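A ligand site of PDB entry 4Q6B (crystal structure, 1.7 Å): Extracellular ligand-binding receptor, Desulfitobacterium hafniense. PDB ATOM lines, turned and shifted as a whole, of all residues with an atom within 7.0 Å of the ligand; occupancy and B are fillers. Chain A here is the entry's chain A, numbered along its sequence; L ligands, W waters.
Arg 82 touches the ligand. CA of Asn 83 touches O1 of the ligand, at 3.5 Å. Ser 106 touches the ligand. Ser 232 touches the ligand. OH of Tyr 285 touches C5 of the ligand (3.1 Å). Hydrophobic or aromatic side chains that line the ligand: Tyr 285. Within 4 Å of the ligand: Arg 82, Asn 83, Ser 84, Ala 105, Ser 106, Thr 107, Asn 231, Ser 232 and Tyr 285.
The backbone NH of Ser 84 is in hydrogen-bond range of the side-chain hydroxyl of Ser 106, 3.5 Å away. The backbone NH (N) of Ser 108 lies within hydrogen-bond range of the side-chain hydroxyl (OG) of Ser 84. The side-chain carboxylate of Asp 126 lies within hydrogen-bond range of the side-chain hydroxyl of Thr 107, 2.6 Å away. OG of Ser 103 sits at hydrogen-bond distance from N of Ala 105, 3.2 Å away. O of Asn 83 lies close to OG of Ser 106, 3.5 Å away. The side-chain hydroxyl (OG) of Ser 106 lies within hydrogen-bond range of the backbone carbonyl oxygen (O) of Arg 82, 2.8 Å away. The backbone carbonyl oxygen (O) of Ser 106 lies within hydrogen-bond range of the guanidinium group (NH2) of Arg 121, 2.8 Å away. The backbone NH (N) of Ser 106 lies within hydrogen-bond range of the side-chain hydroxyl (OG) of Ser 103 (3.0 Å).
An oxygen (O1) of the ligand sits at hydrogen-bond distance from the backbone NH (N) of Ser 84. OG of Ser 84 sits at hydrogen-bond distance from O2 of the ligand, 2.6 Å away. The backbone NH (N) of Thr 107 lies within hydrogen-bond range of an oxygen (O2) of the ligand. The side-chain hydroxyl (OG1) of Thr 107 is in hydrogen-bond range of a nitrogen (N1) of the ligand (3.0 Å). The backbone carbonyl oxygen of Ala 105 is in hydrogen-bond range of a nitrogen (N1) of the ligand. A nitrogen (N1) of the ligand is in hydrogen-bond range of the side-chain amide oxygen (OD1) of Asn 231, at 3.0 Å.
Water W1 lies within hydrogen-bond range of an oxygen (O1) of the ligand (2.6 Å) and the side-chain amide nitrogen (ND2) of Asn 83 (2.9 Å). Water W2 lies within hydrogen-bond range of N of Phe 85 (3.0 Å), O1 of the ligand (3.2 Å) and N of Ser 84 (3.3 Å). Water W3 lies within hydrogen-bond range of the side-chain carboxylate of Asp 126 (2.8 Å), the side-chain hydroxyl of Thr 107 (3.2 Å), an oxygen (O2) of the ligand (3.4 Å) and the backbone NH of Ser 108 (3.5 Å).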
ATOM      1  N   TRP A  17     -18.866 -12.906  19.505  1.00  0.00           N
ATOM      2  CA  TRP A  17     -18.003 -11.885  20.099  1.00  0.00           C
ATOM      3  C   TRP A  17     -17.366 -11.084  19.020  1.00  0.00           C
ATOM      4  O   TRP A  17     -17.273 -11.575  17.903  1.00  0.00           O
ATOM      5  CB  TRP A  17     -16.862 -12.568  20.913  1.00  0.00           C
ATOM      6  CG  TRP A  17     -16.163 -11.716  21.924  1.00  0.00           C
ATOM      7  CD1 TRP A  17     -14.913 -11.218  21.825  1.00  0.00           C
ATOM      8  CD2 TRP A  17     -16.662 -11.342  23.213  1.00  0.00           C
ATOM      9  NE1 TRP A  17     -14.581 -10.508  22.993  1.00  0.00           N
ATOM     10  CE2 TRP A  17     -15.651 -10.581  23.858  1.00  0.00           C
ATOM     11  CE3 TRP A  17     -17.874 -11.603  23.902  1.00  0.00           C
ATOM     12  CZ2 TRP A  17     -15.800 -10.067  25.158  1.00  0.00           C
ATOM     13  CZ3 TRP A  17     -18.029 -11.088  25.195  1.00  0.00           C
ATOM     14  CH2 TRP A  17     -16.996 -10.334  25.803  1.00  0.00           C
ATOM     15  N   ARG A  82     -21.231  -9.340  23.533  1.00  0.00           N
ATOM     16  CA  ARG A  82     -20.428  -8.435  24.387  1.00  0.00           C
ATOM     17  C   ARG A  82     -21.245  -7.189  24.696  1.00  0.00           C
ATOM     18  O   ARG A  82     -21.460  -6.840  25.878  1.00  0.00           O
ATOM     19  CB  ARG A  82     -19.164  -7.986  23.653  1.00  0.00           C
ATOM     20  CG  ARG A  82     -18.214  -7.152  24.521  1.00  0.00           C
ATOM     21  CD  ARG A  82     -16.942  -6.796  23.722  1.00  0.00           C
ATOM     22  NE  ARG A  82     -15.929  -6.044  24.474  1.00  0.00           N
ATOM     23  CZ  ARG A  82     -15.800  -4.722  24.426  1.00  0.00           C
ATOM     24  NH1 ARG A  82     -14.841  -4.134  25.133  1.00  0.00           N
ATOM     25  NH2 ARG A  82     -16.625  -4.003  23.681  1.00  0.00           N
ATOM     26  N   ASN A  83     -21.751  -6.551  23.661  1.00  0.00           N
ATOM     27  CA  ASN A  83     -22.396  -5.252  23.859  1.00  0.00           C
ATOM     28  C   ASN A  83     -23.847  -5.456  24.270  1.00  0.00           C
ATOM     29  O   ASN A  83     -24.548  -6.263  23.643  1.00  0.00           O
ATOM     30  CB  ASN A  83     -22.408  -4.438  22.537  1.00  0.00           C
ATOM     31  CG  ASN A  83     -21.009  -4.183  22.017  1.00  0.00           C
ATOM     32  OD1 ASN A  83     -20.440  -5.040  21.343  1.00  0.00           O
ATOM     33  ND2 ASN A  83     -20.432  -3.014  22.351  1.00  0.00           N
ATOM     34  N   SER A  84     -24.309  -4.736  25.277  1.00  0.00           N
ATOM     35  CA  SER A  84     -25.724  -4.893  25.649  1.00  0.00           C
ATOM     36  C   SER A  84     -26.720  -4.548  24.542  1.00  0.00           C
ATOM     37  O   SER A  84     -27.783  -5.176  24.457  1.00  0.00           O
ATOM     38  CB  SER A  84     -26.043  -4.048  26.904  1.00  0.00           C
ATOM     39  OG  SER A  84     -25.351  -4.536  28.039  1.00  0.00           O
ATOM     40  N   PHE A  85     -26.414  -3.589  23.666  1.00  0.00           N
ATOM     41  CA  PHE A  85     -27.388  -3.283  22.601  1.00  0.00           C
ATOM     42  C   PHE A  85     -27.558  -4.389  21.572  1.00  0.00           C
ATOM     43  O   PHE A  85     -28.527  -4.374  20.784  1.00  0.00           O
ATOM     44  CB  PHE A  85     -27.084  -1.953  21.930  1.00  0.00           C
ATOM     45  CG  PHE A  85     -25.971  -2.039  20.900  1.00  0.00           C
ATOM     46  CD1 PHE A  85     -26.273  -2.212  19.559  1.00  0.00           C
ATOM     47  CD2 PHE A  85     -24.641  -1.925  21.283  1.00  0.00           C
ATOM     48  CE1 PHE A  85     -25.272  -2.281  18.596  1.00  0.00           C
ATOM     49  CE2 PHE A  85     -23.618  -2.008  20.297  1.00  0.00           C
ATOM     50  CZ  PHE A  85     -23.956  -2.193  18.974  1.00  0.00           C
ATOM     51  N   ILE A  86     -26.624  -5.339  21.576  1.00  0.00           N
ATOM     52  CA  ILE A  86     -26.752  -6.572  20.790  1.00  0.00           C
ATOM     53  C   ILE A  86     -27.312  -7.705  21.627  1.00  0.00           C
ATOM     54  O   ILE A  86     -28.257  -8.373  21.214  1.00  0.00           O
ATOM     55  CB  ILE A  86     -25.391  -6.920  20.160  1.00  0.00           C
ATOM     56  CG1 ILE A  86     -24.895  -5.702  19.386  1.00  0.00           C
ATOM     57  CG2 ILE A  86     -25.477  -8.226  19.295  1.00  0.00           C
ATOM     58  CD1 ILE A  86     -23.631  -5.999  18.592  1.00  0.00           C
ATOM     59  N   SER A 103     -23.984 -14.237  28.820  1.00  0.00           N
ATOM     60  CA  SER A 103     -23.116 -13.136  28.463  1.00  0.00           C
ATOM     61  C   SER A 103     -22.048 -12.861  29.497  1.00  0.00           C
ATOM     62  O   SER A 103     -22.300 -12.672  30.659  1.00  0.00           O
ATOM     63  CB  SER A 103     -23.872 -11.828  28.211  1.00  0.00           C
ATOM     64  OG  SER A 103     -22.954 -10.813  27.849  1.00  0.00           O
ATOM     65  N   PRO A 104     -20.760 -12.859  28.942  1.00  0.00           N
ATOM     66  CA  PRO A 104     -19.713 -12.510  29.912  1.00  0.00           C
ATOM     67  C   PRO A 104     -19.343 -11.035  29.885  1.00  0.00           C
ATOM     68  O   PRO A 104     -18.310 -10.686  30.423  1.00  0.00           O
ATOM     69  CB  PRO A 104     -18.539 -13.371  29.455  1.00  0.00           C
ATOM     70  CG  PRO A 104     -18.593 -13.277  27.993  1.00  0.00           C
ATOM     71  CD  PRO A 104     -20.035 -13.224  27.621  1.00  0.00           C
ATOM     72  N   ALA A 105     -20.084 -10.196  29.177  1.00  0.00           N
ATOM     73  CA  ALA A 105     -19.793  -8.778  29.201  1.00  0.00           C
ATOM     74  C   ALA A 105     -20.940  -7.757  29.270  1.00  0.00           C
ATOM     75  O   ALA A 105     -20.696  -6.610  29.584  1.00  0.00           O
ATOM     76  CB  ALA A 105     -18.852  -8.427  28.062  1.00  0.00           C
ATOM     77  N   SER A 106     -22.158  -8.170  28.966  1.00  0.00           N
ATOM     78  CA  SER A 106     -23.229  -7.187  28.846  1.00  0.00           C
ATOM     79  C   SER A 106     -23.789  -6.867  30.212  1.00  0.00           C
ATOM     80  O   SER A 106     -24.387  -7.711  30.842  1.00  0.00           O
ATOM     81  CB  SER A 106     -24.355  -7.724  27.946  1.00  0.00           C
ATOM     82  OG  SER A 106     -23.909  -7.926  26.613  1.00  0.00           O
ATOM     83  N   THR A 107     -23.630  -5.612  30.624  1.00  0.00           N
ATOM     84  CA  THR A 107     -23.944  -5.199  31.994  1.00  0.00           C
ATOM     85  C   THR A 107     -25.242  -4.399  32.142  1.00  0.00           C
ATOM     86  O   THR A 107     -25.635  -4.105  33.275  1.00  0.00           O
ATOM     87  CB  THR A 107     -22.808  -4.334  32.580  1.00  0.00           C
ATOM     88  OG1 THR A 107     -22.585  -3.216  31.686  1.00  0.00           O
ATOM     89  CG2 THR A 107     -21.523  -5.150  32.720  1.00  0.00           C
ATOM     90  N   SER A 108     -25.943  -4.096  31.054  1.00  0.00           N
ATOM     91  CA  SER A 108     -27.215  -3.376  31.191  1.00  0.00           C
ATOM     92  C   SER A 108     -28.234  -4.103  32.060  1.00  0.00           C
ATOM     93  O   SER A 108     -28.556  -5.278  31.830  1.00  0.00           O
ATOM     94  CB  SER A 108     -27.853  -3.133  29.837  1.00  0.00           C
ATOM     95  OG  SER A 108     -29.155  -2.499  30.001  1.00  0.00           O
ATOM     96  N   ARG A 121     -26.138 -13.740  32.619  1.00  0.00           N
ATOM     97  CA  ARG A 121     -24.793 -13.172  32.482  1.00  0.00           C
ATOM     98  C   ARG A 121     -24.023 -13.618  33.661  1.00  0.00           C
ATOM     99  O   ARG A 121     -24.627 -13.877  34.690  1.00  0.00           O
ATOM    100  CB  ARG A 121     -24.830 -11.656  32.445  1.00  0.00           C
ATOM    101  CG  ARG A 121     -25.667 -11.044  33.539  1.00  0.00           C
ATOM    102  CD  ARG A 121     -25.411  -9.513  33.616  1.00  0.00           C
ATOM    103  NE  ARG A 121     -26.649  -8.890  34.093  1.00  0.00           N
ATOM    104  CZ  ARG A 121     -27.284  -7.920  33.460  1.00  0.00           C
ATOM    105  NH1 ARG A 121     -28.453  -7.468  33.925  1.00  0.00           N
ATOM    106  NH2 ARG A 121     -26.762  -7.391  32.360  1.00  0.00           N
ATOM    107  N   ILE A 123     -21.488 -11.906  35.120  1.00  0.00           N
ATOM    108  CA  ILE A 123     -20.752 -10.749  35.636  1.00  0.00           C
ATOM    109  C   ILE A 123     -21.788  -9.858  36.315  1.00  0.00           C
ATOM    110  O   ILE A 123     -22.995  -9.974  36.024  1.00  0.00           O
ATOM    111  CB  ILE A 123     -20.044 -10.006  34.494  1.00  0.00           C
ATOM    112  CG1 ILE A 123     -21.055  -9.591  33.399  1.00  0.00           C
ATOM    113  CG2 ILE A 123     -18.954 -10.916  33.844  1.00  0.00           C
ATOM    114  CD1 ILE A 123     -20.580  -8.470  32.614  1.00  0.00           C
ATOM    115  N   ASP A 126     -24.634  -3.274  35.790  1.00  0.00           N
ATOM    116  CA  ASP A 126     -24.327  -1.852  36.063  1.00  0.00           C
ATOM    117  C   ASP A 126     -24.865  -1.401  37.402  1.00  0.00           C
ATOM    118  O   ASP A 126     -24.254  -0.556  38.052  1.00  0.00           O
ATOM    119  CB  ASP A 126     -24.940  -0.927  34.998  1.00  0.00           C
ATOM    120  CG  ASP A 126     -24.305  -1.083  33.645  1.00  0.00           C
ATOM    121  OD1 ASP A 126     -23.117  -1.487  33.573  1.00  0.00           O
ATOM    122  OD2 ASP A 126     -25.015  -0.809  32.629  1.00  0.00           O
ATOM    123  N   TYR A 154     -28.653   3.537  28.232  1.00  0.00           N
ATOM    124  CA  TYR A 154     -27.579   2.988  29.062  1.00  0.00           C
ATOM    125  C   TYR A 154     -26.881   4.016  29.967  1.00  0.00           C
ATOM    126  O   TYR A 154     -26.571   3.733  31.139  1.00  0.00           O
ATOM    127  CB  TYR A 154     -26.587   2.212  28.181  1.00  0.00           C
ATOM    128  CG  TYR A 154     -27.305   1.245  27.237  1.00  0.00           C
ATOM    129  CD1 TYR A 154     -27.775   0.016  27.693  1.00  0.00           C
ATOM    130  CD2 TYR A 154     -27.532   1.578  25.898  1.00  0.00           C
ATOM    131  CE1 TYR A 154     -28.454  -0.853  26.840  1.00  0.00           C
ATOM    132  CE2 TYR A 154     -28.198   0.713  25.047  1.00  0.00           C
ATOM    133  CZ  TYR A 154     -28.660  -0.501  25.526  1.00  0.00           C
ATOM    134  OH  TYR A 154     -29.329  -1.352  24.667  1.00  0.00           O
ATOM    135  N   THR A 206     -19.089   5.375  28.667  1.00  0.00           N
ATOM    136  CA  THR A 206     -18.132   4.328  28.356  1.00  0.00           C
ATOM    137  C   THR A 206     -16.821   4.935  27.896  1.00  0.00           C
ATOM    138  O   THR A 206     -16.788   6.068  27.463  1.00  0.00           O
ATOM    139  CB  THR A 206     -18.650   3.390  27.255  1.00  0.00           C
ATOM    140  OG1 THR A 206     -18.813   4.131  26.050  1.00  0.00           O
ATOM    141  CG2 THR A 206     -19.966   2.802  27.652  1.00  0.00           C
ATOM    142  N   THR A 208     -14.817   4.165  25.388  1.00  0.00           N
ATOM    143  CA  THR A 208     -14.834   4.470  23.942  1.00  0.00           C
ATOM    144  C   THR A 208     -15.961   5.413  23.521  1.00  0.00           C
ATOM    145  O   THR A 208     -15.953   5.920  22.405  1.00  0.00           O
ATOM    146  CB  THR A 208     -14.901   3.215  23.039  1.00  0.00           C
ATOM    147  OG1 THR A 208     -16.087   2.465  23.340  1.00  0.00           O
ATOM    148  CG2 THR A 208     -13.669   2.356  23.221  1.00  0.00           C
ATOM    149  N   ASN A 231     -17.406  -0.499  34.171  1.00  0.00           N
ATOM    150  CA  ASN A 231     -16.594  -1.588  33.657  1.00  0.00           C
ATOM    151  C   ASN A 231     -15.949  -1.470  32.273  1.00  0.00           C
ATOM    152  O   ASN A 231     -15.011  -2.236  31.959  1.00  0.00           O
ATOM    153  CB  ASN A 231     -17.376  -2.909  33.727  1.00  0.00           C
ATOM    154  CG  ASN A 231     -17.975  -3.287  32.396  1.00  0.00           C
ATOM    155  OD1 ASN A 231     -18.891  -2.633  31.906  1.00  0.00           O
ATOM    156  ND2 ASN A 231     -17.445  -4.335  31.781  1.00  0.00           N
ATOM    157  N   SER A 232     -16.443  -0.562  31.412  1.00  0.00           N
ATOM    158  CA  SER A 232     -15.823  -0.442  30.093  1.00  0.00           C
ATOM    159  C   SER A 232     -14.403   0.135  30.192  1.00  0.00           C
ATOM    160  O   SER A 232     -13.628   0.129  29.219  1.00  0.00           O
ATOM    161  CB  SER A 232     -16.676   0.463  29.183  1.00  0.00           C
ATOM    162  OG  SER A 232     -16.885   1.703  29.804  1.00  0.00           O
ATOM    163  N   TRP A 233     -14.064   0.626  31.372  1.00  0.00           N
ATOM    164  CA  TRP A 233     -12.766   1.271  31.613  1.00  0.00           C
ATOM    165  C   TRP A 233     -11.699   0.255  32.037  1.00  0.00           C
ATOM    166  O   TRP A 233     -10.516   0.598  32.112  1.00  0.00           O
ATOM    167  CB  TRP A 233     -12.916   2.375  32.641  1.00  0.00           C
ATOM    168  CG  TRP A 233     -13.735   3.544  32.134  1.00  0.00           C
ATOM    169  CD1 TRP A 233     -15.090   3.587  31.954  1.00  0.00           C
ATOM    170  CD2 TRP A 233     -13.243   4.839  31.792  1.00  0.00           C
ATOM    171  NE1 TRP A 233     -15.474   4.827  31.491  1.00  0.00           N
ATOM    172  CE2 TRP A 233     -14.357   5.613  31.386  1.00  0.00           C
ATOM    173  CE3 TRP A 233     -11.969   5.401  31.750  1.00  0.00           C
ATOM    174  CZ2 TRP A 233     -14.220   6.954  30.973  1.00  0.00           C
ATOM    175  CZ3 TRP A 233     -11.845   6.716  31.331  1.00  0.00           C
ATOM    176  CH2 TRP A 233     -12.972   7.472  30.947  1.00  0.00           C
ATOM    177  N   ALA A 235     -11.090  -2.486  30.124  1.00  0.00           N
ATOM    178  CA  ALA A 235     -10.488  -2.611  28.780  1.00  0.00           C
ATOM    179  C   ALA A 235      -9.668  -1.378  28.367  1.00  0.00           C
ATOM    180  O   ALA A 235      -9.522  -1.084  27.167  1.00  0.00           O
ATOM    181  CB  ALA A 235     -11.583  -2.900  27.755  1.00  0.00           C
ATOM    182  N   PHE A 257     -14.800  -6.326  37.487  1.00  0.00           N
ATOM    183  CA  PHE A 257     -14.804  -7.671  38.024  1.00  0.00           C
ATOM    184  C   PHE A 257     -13.493  -8.398  37.682  1.00  0.00           C
ATOM    185  O   PHE A 257     -12.742  -7.970  36.820  1.00  0.00           O
ATOM    186  CB  PHE A 257     -16.005  -8.452  37.501  1.00  0.00           C
ATOM    187  CG  PHE A 257     -16.100  -8.480  36.015  1.00  0.00           C
ATOM    188  CD1 PHE A 257     -16.880  -7.579  35.341  1.00  0.00           C
ATOM    189  CD2 PHE A 257     -15.365  -9.395  35.299  1.00  0.00           C
ATOM    190  CE1 PHE A 257     -16.932  -7.582  33.972  1.00  0.00           C
ATOM    191  CE2 PHE A 257     -15.417  -9.398  33.930  1.00  0.00           C
ATOM    192  CZ  PHE A 257     -16.204  -8.502  33.261  1.00  0.00           C
ATOM    193  N   TYR A 285     -11.946 -10.122  30.870  1.00  0.00           N
ATOM    194  CA  TYR A 285     -12.732 -10.865  29.862  1.00  0.00           C
ATOM    195  C   TYR A 285     -12.277 -12.309  29.640  1.00  0.00           C
ATOM    196  O   TYR A 285     -13.120 -13.221  29.463  1.00  0.00           O
ATOM    197  CB  TYR A 285     -12.734 -10.098  28.523  1.00  0.00           C
ATOM    198  CG  TYR A 285     -13.283  -8.705  28.729  1.00  0.00           C
ATOM    199  CD1 TYR A 285     -14.619  -8.500  29.019  1.00  0.00           C
ATOM    200  CD2 TYR A 285     -12.415  -7.610  28.761  1.00  0.00           C
ATOM    201  CE1 TYR A 285     -15.120  -7.204  29.260  1.00  0.00           C
ATOM    202  CE2 TYR A 285     -12.887  -6.336  28.998  1.00  0.00           C
ATOM    203  CZ  TYR A 285     -14.231  -6.138  29.252  1.00  0.00           C
ATOM    204  OH  TYR A 285     -14.672  -4.842  29.491  1.00  0.00           O
HETATM  205  N1  LIG L   1     -20.503  -3.592  29.505  1.00  0.00           N
HETATM  206  C1  LIG L   1     -20.621  -3.172  28.105  1.00  0.00           C
HETATM  207  C2  LIG L   1     -22.047  -3.357  27.607  1.00  0.00           C
HETATM  208  O1  LIG L   1     -22.382  -2.991  26.487  1.00  0.00           O
HETATM  209  C3  LIG L   1     -19.653  -3.978  27.241  1.00  0.00           C
HETATM  210  C4  LIG L   1     -18.267  -3.508  27.716  1.00  0.00           C
HETATM  211  C5  LIG L   1     -17.374  -4.672  28.000  1.00  0.00           C
HETATM  212  C6  LIG L   1     -17.607  -2.508  26.774  1.00  0.00           C
HETATM  213  O2  LIG L   1     -22.888  -3.864  28.373  1.00  0.00           O
HETATM  214  O   HOH W   1     -21.500  -1.471  24.536  1.00  0.00           O
HETATM  215  O   HOH W   2     -24.691  -1.461  24.843  1.00  0.00           O
HETATM  216  O   HOH W   3     -24.345  -1.191  29.940  1.00  0.00           O
